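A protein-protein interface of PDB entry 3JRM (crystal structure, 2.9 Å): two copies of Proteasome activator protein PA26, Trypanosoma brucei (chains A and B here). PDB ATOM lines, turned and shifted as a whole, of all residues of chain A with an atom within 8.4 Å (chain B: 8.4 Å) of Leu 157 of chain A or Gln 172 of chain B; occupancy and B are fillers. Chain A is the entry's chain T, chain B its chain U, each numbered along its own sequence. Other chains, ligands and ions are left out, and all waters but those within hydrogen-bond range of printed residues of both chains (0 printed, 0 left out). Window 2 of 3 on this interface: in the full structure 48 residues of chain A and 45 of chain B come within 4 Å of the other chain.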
ATOM      1  N   GLY A  53       1.807  -9.241  19.085  1.00  0.00           N
ATOM      2  CA  GLY A  53       2.864  -9.232  18.096  1.00  0.00           C
ATOM      3  C   GLY A  53       4.081  -9.880  18.713  1.00  0.00           C
ATOM      4  O   GLY A  53       4.054 -10.297  19.874  1.00  0.00           O
ATOM      5  N   ARG A  54       5.145  -9.956  17.925  1.00  0.00           N
ATOM      6  CA  ARG A  54       6.436 -10.459  18.368  1.00  0.00           C
ATOM      7  C   ARG A  54       6.921  -9.798  19.661  1.00  0.00           C
ATOM      8  O   ARG A  54       7.668 -10.414  20.414  1.00  0.00           O
ATOM      9  CB  ARG A  54       7.455 -10.241  17.246  1.00  0.00           C
ATOM     10  CG  ARG A  54       8.788 -10.940  17.413  1.00  0.00           C
ATOM     11  CD  ARG A  54       9.946 -10.023  16.934  1.00  0.00           C
ATOM     12  NE  ARG A  54      11.248 -10.526  17.376  1.00  0.00           N
ATOM     13  CZ  ARG A  54      11.859 -11.589  16.858  1.00  0.00           C
ATOM     14  NH1 ARG A  54      11.306 -12.283  15.855  1.00  0.00           N
ATOM     15  NH2 ARG A  54      13.033 -11.968  17.360  1.00  0.00           N
ATOM     16  N   ALA A  55       6.515  -8.552  19.921  1.00  0.00           N
ATOM     17  CA  ALA A  55       6.834  -7.886  21.193  1.00  0.00           C
ATOM     18  C   ALA A  55       6.463  -8.752  22.414  1.00  0.00           C
ATOM     19  O   ALA A  55       7.194  -8.783  23.409  1.00  0.00           O
ATOM     20  CB  ALA A  55       6.138  -6.530  21.274  1.00  0.00           C
ATOM     21  N   GLN A  56       5.335  -9.467  22.329  1.00  0.00           N
ATOM     22  CA  GLN A  56       4.832 -10.262  23.455  1.00  0.00           C
ATOM     23  C   GLN A  56       5.674 -11.504  23.735  1.00  0.00           C
ATOM     24  O   GLN A  56       5.664 -12.016  24.844  1.00  0.00           O
ATOM     25  CB  GLN A  56       3.359 -10.642  23.249  1.00  0.00           C
ATOM     26  CG  GLN A  56       2.368  -9.512  23.558  1.00  0.00           C
ATOM     27  CD  GLN A  56       2.632  -8.283  22.715  1.00  0.00           C
ATOM     28  OE1 GLN A  56       2.397  -8.283  21.512  1.00  0.00           O
ATOM     29  NE2 GLN A  56       3.165  -7.244  23.334  1.00  0.00           N
ATOM     30  N   ALA A  57       6.411 -11.985  22.743  1.00  0.00           N
ATOM     31  CA  ALA A  57       7.323 -13.108  22.936  1.00  0.00           C
ATOM     32  C   ALA A  57       8.612 -12.685  23.633  1.00  0.00           C
ATOM     33  O   ALA A  57       9.424 -13.524  24.013  1.00  0.00           O
ATOM     34  CB  ALA A  57       7.656 -13.746  21.614  1.00  0.00           C
ATOM     35  N   GLU A  58       8.809 -11.383  23.797  1.00  0.00           N
ATOM     36  CA  GLU A  58      10.047 -10.858  24.385  1.00  0.00           C
ATOM     37  C   GLU A  58       9.958 -10.534  25.882  1.00  0.00           C
ATOM     38  O   GLU A  58      10.967 -10.276  26.503  1.00  0.00           O
ATOM     39  CB  GLU A  58      10.497  -9.615  23.614  1.00  0.00           C
ATOM     40  CG  GLU A  58      11.375  -9.902  22.399  1.00  0.00           C
ATOM     41  CD  GLU A  58      11.383  -8.759  21.389  1.00  0.00           C
ATOM     42  OE1 GLU A  58      10.993  -7.638  21.770  1.00  0.00           O
ATOM     43  OE2 GLU A  58      11.770  -8.990  20.213  1.00  0.00           O
ATOM     44  N   LYS A  59       8.763 -10.565  26.455  1.00  0.00           N
ATOM     45  CA  LYS A  59       8.573 -10.368  27.899  1.00  0.00           C
ATOM     46  C   LYS A  59       7.498 -11.328  28.455  1.00  0.00           C
ATOM     47  O   LYS A  59       6.477 -11.551  27.801  1.00  0.00           O
ATOM     48  CB  LYS A  59       8.173  -8.915  28.161  1.00  0.00           C
ATOM     49  CG  LYS A  59       8.195  -8.505  29.639  1.00  0.00           C
ATOM     50  CD  LYS A  59       8.101  -6.972  29.822  1.00  0.00           C
ATOM     51  CE  LYS A  59       8.930  -6.469  31.052  1.00  0.00           C
ATOM     52  NZ  LYS A  59       8.686  -7.241  32.321  1.00  0.00           N
ATOM     53  N   ARG A 149       4.950 -21.665  27.493  1.00  0.00           N
ATOM     54  CA  ARG A 149       5.187 -20.370  26.880  1.00  0.00           C
ATOM     55  C   ARG A 149       6.567 -20.268  26.286  1.00  0.00           C
ATOM     56  O   ARG A 149       6.724 -19.715  25.210  1.00  0.00           O
ATOM     57  CB  ARG A 149       4.981 -19.226  27.867  1.00  0.00           C
ATOM     58  CG  ARG A 149       4.617 -17.895  27.203  1.00  0.00           C
ATOM     59  CD  ARG A 149       4.423 -16.785  28.223  1.00  0.00           C
ATOM     60  NE  ARG A 149       3.642 -15.687  27.672  1.00  0.00           N
ATOM     61  CZ  ARG A 149       4.107 -14.696  26.912  1.00  0.00           C
ATOM     62  NH1 ARG A 149       5.383 -14.611  26.595  1.00  0.00           N
ATOM     63  NH2 ARG A 149       3.263 -13.775  26.470  1.00  0.00           N
ATOM     64  N   SER A 150       7.572 -20.787  26.977  1.00  0.00           N
ATOM     65  CA  SER A 150       8.950 -20.682  26.482  1.00  0.00           C
ATOM     66  C   SER A 150       9.151 -21.457  25.175  1.00  0.00           C
ATOM     67  O   SER A 150       9.913 -21.027  24.320  1.00  0.00           O
ATOM     68  CB  SER A 150       9.983 -21.096  27.542  1.00  0.00           C
ATOM     69  OG  SER A 150       9.936 -22.472  27.818  1.00  0.00           O
ATOM     70  N   THR A 151       8.465 -22.582  25.009  1.00  0.00           N
ATOM     71  CA  THR A 151       8.585 -23.339  23.763  1.00  0.00           C
ATOM     72  C   THR A 151       8.108 -22.475  22.606  1.00  0.00           C
ATOM     73  O   THR A 151       8.736 -22.439  21.563  1.00  0.00           O
ATOM     74  CB  THR A 151       7.776 -24.660  23.792  1.00  0.00           C
ATOM     75  OG1 THR A 151       8.248 -25.496  24.851  1.00  0.00           O
ATOM     76  CG2 THR A 151       7.928 -25.409  22.479  1.00  0.00           C
ATOM     77  N   VAL A 152       7.000 -21.776  22.808  1.00  0.00           N
ATOM     78  CA  VAL A 152       6.415 -20.949  21.772  1.00  0.00           C
ATOM     79  C   VAL A 152       7.235 -19.663  21.599  1.00  0.00           C
ATOM     80  O   VAL A 152       7.366 -19.150  20.496  1.00  0.00           O
ATOM     81  CB  VAL A 152       4.891 -20.646  22.059  1.00  0.00           C
ATOM     82  CG1 VAL A 152       4.322 -19.601  21.094  1.00  0.00           C
ATOM     83  CG2 VAL A 152       4.056 -21.923  21.969  1.00  0.00           C
ATOM     84  N   GLU A 153       7.777 -19.138  22.691  1.00  0.00           N
ATOM     85  CA  GLU A 153       8.695 -17.986  22.632  1.00  0.00           C
ATOM     86  C   GLU A 153       9.928 -18.278  21.794  1.00  0.00           C
ATOM     87  O   GLU A 153      10.325 -17.474  20.965  1.00  0.00           O
ATOM     88  CB  GLU A 153       9.135 -17.582  24.024  1.00  0.00           C
ATOM     89  CG  GLU A 153       8.051 -16.870  24.794  1.00  0.00           C
ATOM     90  CD  GLU A 153       8.400 -16.687  26.253  1.00  0.00           C
ATOM     91  OE1 GLU A 153       9.531 -17.052  26.650  1.00  0.00           O
ATOM     92  OE2 GLU A 153       7.542 -16.163  27.003  1.00  0.00           O
ATOM     93  N   ASP A 154      10.529 -19.440  22.003  1.00  0.00           N
ATOM     94  CA  ASP A 154      11.671 -19.847  21.196  1.00  0.00           C
ATOM     95  C   ASP A 154      11.329 -19.852  19.729  1.00  0.00           C
ATOM     96  O   ASP A 154      12.007 -19.188  18.957  1.00  0.00           O
ATOM     97  CB  ASP A 154      12.210 -21.229  21.595  1.00  0.00           C
ATOM     98  CG  ASP A 154      13.471 -21.136  22.421  1.00  0.00           C
ATOM     99  OD1 ASP A 154      13.663 -20.114  23.096  1.00  0.00           O
ATOM    100  OD2 ASP A 154      14.282 -22.079  22.409  1.00  0.00           O
ATOM    101  N   LYS A 155      10.283 -20.584  19.337  1.00  0.00           N
ATOM    102  CA  LYS A 155       9.948 -20.710  17.920  1.00  0.00           C
ATOM    103  C   LYS A 155       9.698 -19.357  17.287  1.00  0.00           C
ATOM    104  O   LYS A 155      10.080 -19.148  16.153  1.00  0.00           O
ATOM    105  CB  LYS A 155       8.740 -21.612  17.717  1.00  0.00           C
ATOM    106  CG  LYS A 155       8.990 -23.072  18.104  1.00  0.00           C
ATOM    107  CD  LYS A 155       7.739 -23.938  17.926  1.00  0.00           C
ATOM    108  CE  LYS A 155       8.039 -25.402  18.183  1.00  0.00           C
ATOM    109  NZ  LYS A 155       7.296 -26.233  17.218  1.00  0.00           N
ATOM    110  N   LEU A 156       9.092 -18.436  18.035  1.00  0.00           N
ATOM    111  CA  LEU A 156       8.777 -17.098  17.524  1.00  0.00           C
ATOM    112  C   LEU A 156      10.019 -16.198  17.412  1.00  0.00           C
ATOM    113  O   LEU A 156      10.147 -15.432  16.465  1.00  0.00           O
ATOM    114  CB  LEU A 156       7.700 -16.408  18.384  1.00  0.00           C
ATOM    115  CG  LEU A 156       6.255 -16.903  18.275  1.00  0.00           C
ATOM    116  CD1 LEU A 156       5.374 -16.175  19.293  1.00  0.00           C
ATOM    117  CD2 LEU A 156       5.714 -16.731  16.876  1.00  0.00           C
ATOM    118  N   LEU A 157      10.918 -16.281  18.387  1.00  0.00           N
ATOM    119  CA  LEU A 157      12.120 -15.431  18.415  1.00  0.00           C
ATOM    120  C   LEU A 157      13.249 -15.998  17.544  1.00  0.00           C
ATOM    121  O   LEU A 157      13.803 -15.301  16.716  1.00  0.00           O
ATOM    122  CB  LEU A 157      12.622 -15.234  19.860  1.00  0.00           C
ATOM    123  CG  LEU A 157      11.697 -14.553  20.869  1.00  0.00           C
ATOM    124  CD1 LEU A 157      12.315 -14.598  22.248  1.00  0.00           C
ATOM    125  CD2 LEU A 157      11.383 -13.118  20.465  1.00  0.00           C
ATOM    126  N   GLY A 158      13.584 -17.264  17.738  1.00  0.00           N
ATOM    127  CA  GLY A 158      14.739 -17.865  17.080  1.00  0.00           C
ATOM    128  C   GLY A 158      16.003 -17.638  17.877  1.00  0.00           C
ATOM    129  O   GLY A 158      17.034 -18.245  17.585  1.00  0.00           O
ATOM    130  N   GLY A 169      16.025 -16.519  12.733  1.00  0.00           N
ATOM    131  CA  GLY A 169      14.740 -16.188  12.111  1.00  0.00           C
ATOM    132  C   GLY A 169      13.556 -16.887  12.779  1.00  0.00           C
ATOM    133  O   GLY A 169      13.490 -18.126  12.821  1.00  0.00           O
ATOM    134  N   GLY A 170      12.613 -16.093  13.284  1.00  0.00           N
ATOM    135  CA  GLY A 170      11.448 -16.628  13.990  1.00  0.00           C
ATOM    136  C   GLY A 170      10.438 -17.300  13.076  1.00  0.00           C
ATOM    137  O   GLY A 170      10.504 -17.139  11.869  1.00  0.00           O
ATOM    138  N   SER A 171       9.504 -18.059  13.643  1.00  0.00           N
ATOM    139  CA  SER A 171       8.508 -18.734  12.837  1.00  0.00           C
ATOM    140  C   SER A 171       7.592 -17.679  12.230  1.00  0.00           C
ATOM    141  O   SER A 171       7.320 -16.644  12.848  1.00  0.00           O
ATOM    142  CB  SER A 171       7.709 -19.731  13.672  1.00  0.00           C
ATOM    143  OG  SER A 171       6.625 -20.265  12.941  1.00  0.00           O
ATOM    144  N   LEU A 176       0.815 -19.803  15.413  1.00  0.00           N
ATOM    145  CA  LEU A 176       1.764 -19.834  16.529  1.00  0.00           C
ATOM    146  C   LEU A 176       1.737 -18.537  17.342  1.00  0.00           C
ATOM    147  O   LEU A 176       1.822 -18.559  18.561  1.00  0.00           O
ATOM    148  CB  LEU A 176       3.180 -20.103  16.048  1.00  0.00           C
ATOM    149  CG  LEU A 176       4.201 -20.388  17.141  1.00  0.00           C
ATOM    150  CD1 LEU A 176       3.875 -21.683  17.888  1.00  0.00           C
ATOM    151  CD2 LEU A 176       5.610 -20.452  16.540  1.00  0.00           C
ATOM    152  N   LEU A 180       0.528 -18.233  21.429  1.00  0.00           N
ATOM    153  CA  LEU A 180       1.185 -17.561  22.543  1.00  0.00           C
ATOM    154  C   LEU A 180       0.144 -16.827  23.378  1.00  0.00           C
ATOM    155  O   LEU A 180       0.153 -16.894  24.600  1.00  0.00           O
ATOM    156  CB  LEU A 180       2.229 -16.566  22.036  1.00  0.00           C
ATOM    157  CG  LEU A 180       3.009 -15.794  23.103  1.00  0.00           C
ATOM    158  CD1 LEU A 180       3.934 -16.714  23.842  1.00  0.00           C
ATOM    159  CD2 LEU A 180       3.773 -14.676  22.458  1.00  0.00           C
ATOM    160  N   ARG B  54      21.220 -14.832  33.191  1.00  0.00           N
ATOM    161  CA  ARG B  54      22.090 -15.851  32.664  1.00  0.00           C
ATOM    162  C   ARG B  54      23.147 -16.337  33.673  1.00  0.00           C
ATOM    163  O   ARG B  54      23.552 -17.489  33.625  1.00  0.00           O
ATOM    164  CB  ARG B  54      22.760 -15.296  31.412  1.00  0.00           C
ATOM    165  CG  ARG B  54      23.497 -16.325  30.552  1.00  0.00           C
ATOM    166  CD  ARG B  54      24.802 -15.714  29.980  1.00  0.00           C
ATOM    167  NE  ARG B  54      25.667 -16.752  29.417  1.00  0.00           N
ATOM    168  CZ  ARG B  54      25.443 -17.390  28.264  1.00  0.00           C
ATOM    169  NH1 ARG B  54      24.366 -17.105  27.519  1.00  0.00           N
ATOM    170  NH2 ARG B  54      26.295 -18.329  27.851  1.00  0.00           N
ATOM    171  N   LYS B 155      19.901 -24.926  27.119  1.00  0.00           N
ATOM    172  CA  LYS B 155      19.227 -24.031  26.200  1.00  0.00           C
ATOM    173  C   LYS B 155      19.613 -22.577  26.447  1.00  0.00           C
ATOM    174  O   LYS B 155      19.700 -21.800  25.513  1.00  0.00           O
ATOM    175  CB  LYS B 155      17.715 -24.193  26.280  1.00  0.00           C
ATOM    176  CG  LYS B 155      17.223 -25.569  25.829  1.00  0.00           C
ATOM    177  CD  LYS B 155      15.697 -25.722  25.991  1.00  0.00           C
ATOM    178  CE  LYS B 155      15.197 -27.049  25.408  1.00  0.00           C
ATOM    179  NZ  LYS B 155      13.911 -26.815  24.709  1.00  0.00           N
ATOM    180  N   LEU B 156      19.848 -22.216  27.705  1.00  0.00           N
ATOM    181  CA  LEU B 156      20.175 -20.821  28.054  1.00  0.00           C
ATOM    182  C   LEU B 156      21.625 -20.443  27.731  1.00  0.00           C
ATOM    183  O   LEU B 156      21.902 -19.304  27.333  1.00  0.00           O
ATOM    184  CB  LEU B 156      19.878 -20.532  29.536  1.00  0.00           C
ATOM    185  CG  LEU B 156      18.418 -20.388  29.986  1.00  0.00           C
ATOM    186  CD1 LEU B 156      18.353 -20.233  31.496  1.00  0.00           C
ATOM    187  CD2 LEU B 156      17.704 -19.235  29.315  1.00  0.00           C
ATOM    188  N   GLY B 169      25.047 -19.616  20.986  1.00  0.00           N
ATOM    189  CA  GLY B 169      24.045 -18.603  21.293  1.00  0.00           C
ATOM    190  C   GLY B 169      22.884 -19.160  22.091  1.00  0.00           C
ATOM    191  O   GLY B 169      22.161 -20.042  21.624  1.00  0.00           O
ATOM    192  N   GLY B 170      22.704 -18.635  23.301  1.00  0.00           N
ATOM    193  CA  GLY B 170      21.664 -19.109  24.208  1.00  0.00           C
ATOM    194  C   GLY B 170      20.275 -18.703  23.776  1.00  0.00           C
ATOM    195  O   GLY B 170      20.132 -17.859  22.916  1.00  0.00           O
ATOM    196  N   SER B 171      19.254 -19.313  24.369  1.00  0.00           N
ATOM    197  CA  SER B 171      17.884 -19.006  24.011  1.00  0.00           C
ATOM    198  C   SER B 171      17.556 -17.594  24.462  1.00  0.00           C
ATOM    199  O   SER B 171      18.025 -17.135  25.494  1.00  0.00           O
ATOM    200  CB  SER B 171      16.928 -20.013  24.646  1.00  0.00           C
ATOM    201  OG  SER B 171      15.587 -19.597  24.527  1.00  0.00           O
ATOM    202  N   GLN B 172      16.755 -16.906  23.672  1.00  0.00           N
ATOM    203  CA  GLN B 172      16.288 -15.569  24.005  1.00  0.00           C
ATOM    204  C   GLN B 172      14.917 -15.599  24.693  1.00  0.00           C
ATOM    205  O   GLN B 172      14.287 -14.563  24.858  1.00  0.00           O
ATOM    206  CB  GLN B 172      16.201 -14.717  22.713  1.00  0.00           C
ATOM    207  CG  GLN B 172      17.560 -14.292  22.087  1.00  0.00           C
ATOM    208  CD  GLN B 172      18.305 -13.195  22.910  1.00  0.00           C
ATOM    209  OE1 GLN B 172      18.893 -13.462  23.977  1.00  0.00           O
ATOM    210  NE2 GLN B 172      18.292 -11.968  22.392  1.00  0.00           N
ATOM    211  N   SER B 173      14.447 -16.780  25.091  1.00  0.00           N
ATOM    212  CA  SER B 173      13.121 -16.907  25.677  1.00  0.00           C
ATOM    213  C   SER B 173      13.085 -16.260  27.048  1.00  0.00           C
ATOM    214  O   SER B 173      13.805 -16.677  27.942  1.00  0.00           O
ATOM    215  CB  SER B 173      12.715 -18.376  25.802  1.00  0.00           C
ATOM    216  OG  SER B 173      11.505 -18.502  26.542  1.00  0.00           O
ATOM    217  N   PRO B 174      12.242 -15.242  27.232  1.00  0.00           N
ATOM    218  CA  PRO B 174      12.119 -14.704  28.578  1.00  0.00           C
ATOM    219  C   PRO B 174      11.563 -15.727  29.571  1.00  0.00           C
ATOM    220  O   PRO B 174      12.006 -15.753  30.708  1.00  0.00           O
ATOM    221  CB  PRO B 174      11.159 -13.516  28.407  1.00  0.00           C
ATOM    222  CG  PRO B 174      10.402 -13.824  27.203  1.00  0.00           C
ATOM    223  CD  PRO B 174      11.333 -14.570  26.295  1.00  0.00           C
ATOM    224  N   SER B 175      10.619 -16.558  29.136  1.00  0.00           N
ATOM    225  CA  SER B 175       9.972 -17.515  30.024  1.00  0.00           C
ATOM    226  C   SER B 175      10.911 -18.643  30.393  1.00  0.00           C
ATOM    227  O   SER B 175      10.822 -19.160  31.490  1.00  0.00           O
ATOM    228  CB  SER B 175       8.686 -18.075  29.396  1.00  0.00           C
ATOM    229  OG  SER B 175       7.696 -17.060  29.283  1.00  0.00           O
ATOM    230  N   LEU B 176      11.800 -19.034  29.479  1.00  0.00           N
ATOM    231  CA  LEU B 176      12.801 -20.062  29.781  1.00  0.00           C
ATOM    232  C   LEU B 176      13.676 -19.653  30.963  1.00  0.00           C
ATOM    233  O   LEU B 176      14.019 -20.478  31.803  1.00  0.00           O
ATOM    234  CB  LEU B 176      13.663 -20.395  28.562  1.00  0.00           C
ATOM    235  CG  LEU B 176      14.581 -21.605  28.747  1.00  0.00           C
ATOM    236  CD1 LEU B 176      13.784 -22.906  28.954  1.00  0.00           C
ATOM    237  CD2 LEU B 176      15.535 -21.732  27.577  1.00  0.00           C
ATOM    238  N   LEU B 177      14.021 -18.378  31.040  1.00  0.00           N
ATOM    239  CA  LEU B 177      14.835 -17.870  32.147  1.00  0.00           C
ATOM    240  C   LEU B 177      14.069 -17.982  33.460  1.00  0.00           C
ATOM    241  O   LEU B 177      14.607 -18.469  34.443  1.00  0.00           O
ATOM    242  CB  LEU B 177      15.245 -16.409  31.880  1.00  0.00           C
ATOM    243  CG  LEU B 177      16.288 -15.772  32.788  1.00  0.00           C
ATOM    244  CD1 LEU B 177      17.539 -16.620  32.757  1.00  0.00           C
ATOM    245  CD2 LEU B 177      16.577 -14.390  32.313  1.00  0.00           C
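Positions printed for both chains: 54, 155, 156, 169, 170, 171 and 176.
Among the printed residues, no Asp or Glu carboxylate lies within 4 Å of a Lys or Arg side-chain nitrogen of the other chain.
Pro 174 of chain B touches Ala 57 of chain A (CD to O, 3.2 Å). Pro 174 of chain B touches Glu 58 of chain A (CG to C, 3.6 Å). Lys 59 of chain A touches Pro 174 of chain B. Arg 149 of chain A touches Ser 175 of chain B (CD to OG, 3.5 Å). Ser 150 of chain A touches Ser 173 of chain B (CB to OG, 3.2 Å). Ser 150 of chain A touches Ser 175 of chain B. Ser 150 of chain A touches Leu 176 of chain B. Asp 154 of chain A touches Ser 173 of chain B (OD1 to CB, 3.4 Å). CD1 of Leu 157 of chain A touches O of Gln 172 of chain B, at 3.3 Å.
The guanidinium group of Arg 54 of chain A lies within salt-bridge range of the side-chain carboxylate of Glu 58 of chain A (3.3 Å). The backbone carbonyl oxygen (O) of Gln 56 of chain A sits at hydrogen-bond distance from the guanidinium group (NH1) of Arg 149 of chain A (3.1 Å). NH1 of Arg 149 of chain A lies within salt-bridge range of OE2 of Glu 153 of chain A. OG of Ser 171 of chain B lies within hydrogen-bond range of N of Ser 173 of chain B (3.1 Å). The side-chain hydroxyl (OG) of Ser 173 of chain B lies close to the backbone NH (N) of Ser 175 of chain B (3.4 Å). N of Leu 176 of chain B sits at hydrogen-bond distance from OG of Ser 173 of chain B, at 3.0 Å.
Of the printed residues of chain B, Glu 153 of chain A touches Ser 173 (2.5 Å), Pro 174 (3.1 Å) and Ser 175 (2.5 Å). Leu 157 of chain A touches just one residue of chain B: Gln 172 (3.3 Å). Ser 171 of chain B touches just one residue of chain A: Asp 154. Gln 172 of chain B touches just one residue of chain A: Leu 157. Of the printed residues of chain A, Ser 173 of chain B touches Ser 150, Glu 153 and Asp 154. Printed residues of chain A within 4 Å of Pro 174 of chain B: Ala 57 (3.2 Å), Glu 58 (3.6 Å), Lys 59 (3.7 Å) and Glu 153 (3.1 Å). The nearest residue of chain A that does not touch Gln 172 of chain B is Asp 154 of chain A (4.5 Å). The nearest printed residue of chain A that does not touch Ser 173 of chain B is Leu 157 of chain A (4.2 Å).
OE1 of Glu 153 of chain A is in hydrogen-bond range of OG of Ser 173 of chain B (2.5 Å). The side-chain carboxylate of Glu 153 of chain A lies within hydrogen-bond range of the side-chain hydroxyl of Ser 175 of chain B, at 2.5 Å. OD1 of Asp 154 of chain A lies within hydrogen-bond range of OG of Ser 171 of chain B (2.5 Å). The side-chain carboxylate of Glu 153 of chain A lies close to the backbone nitrogen of Pro 174 of chain B (3.3 Å).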
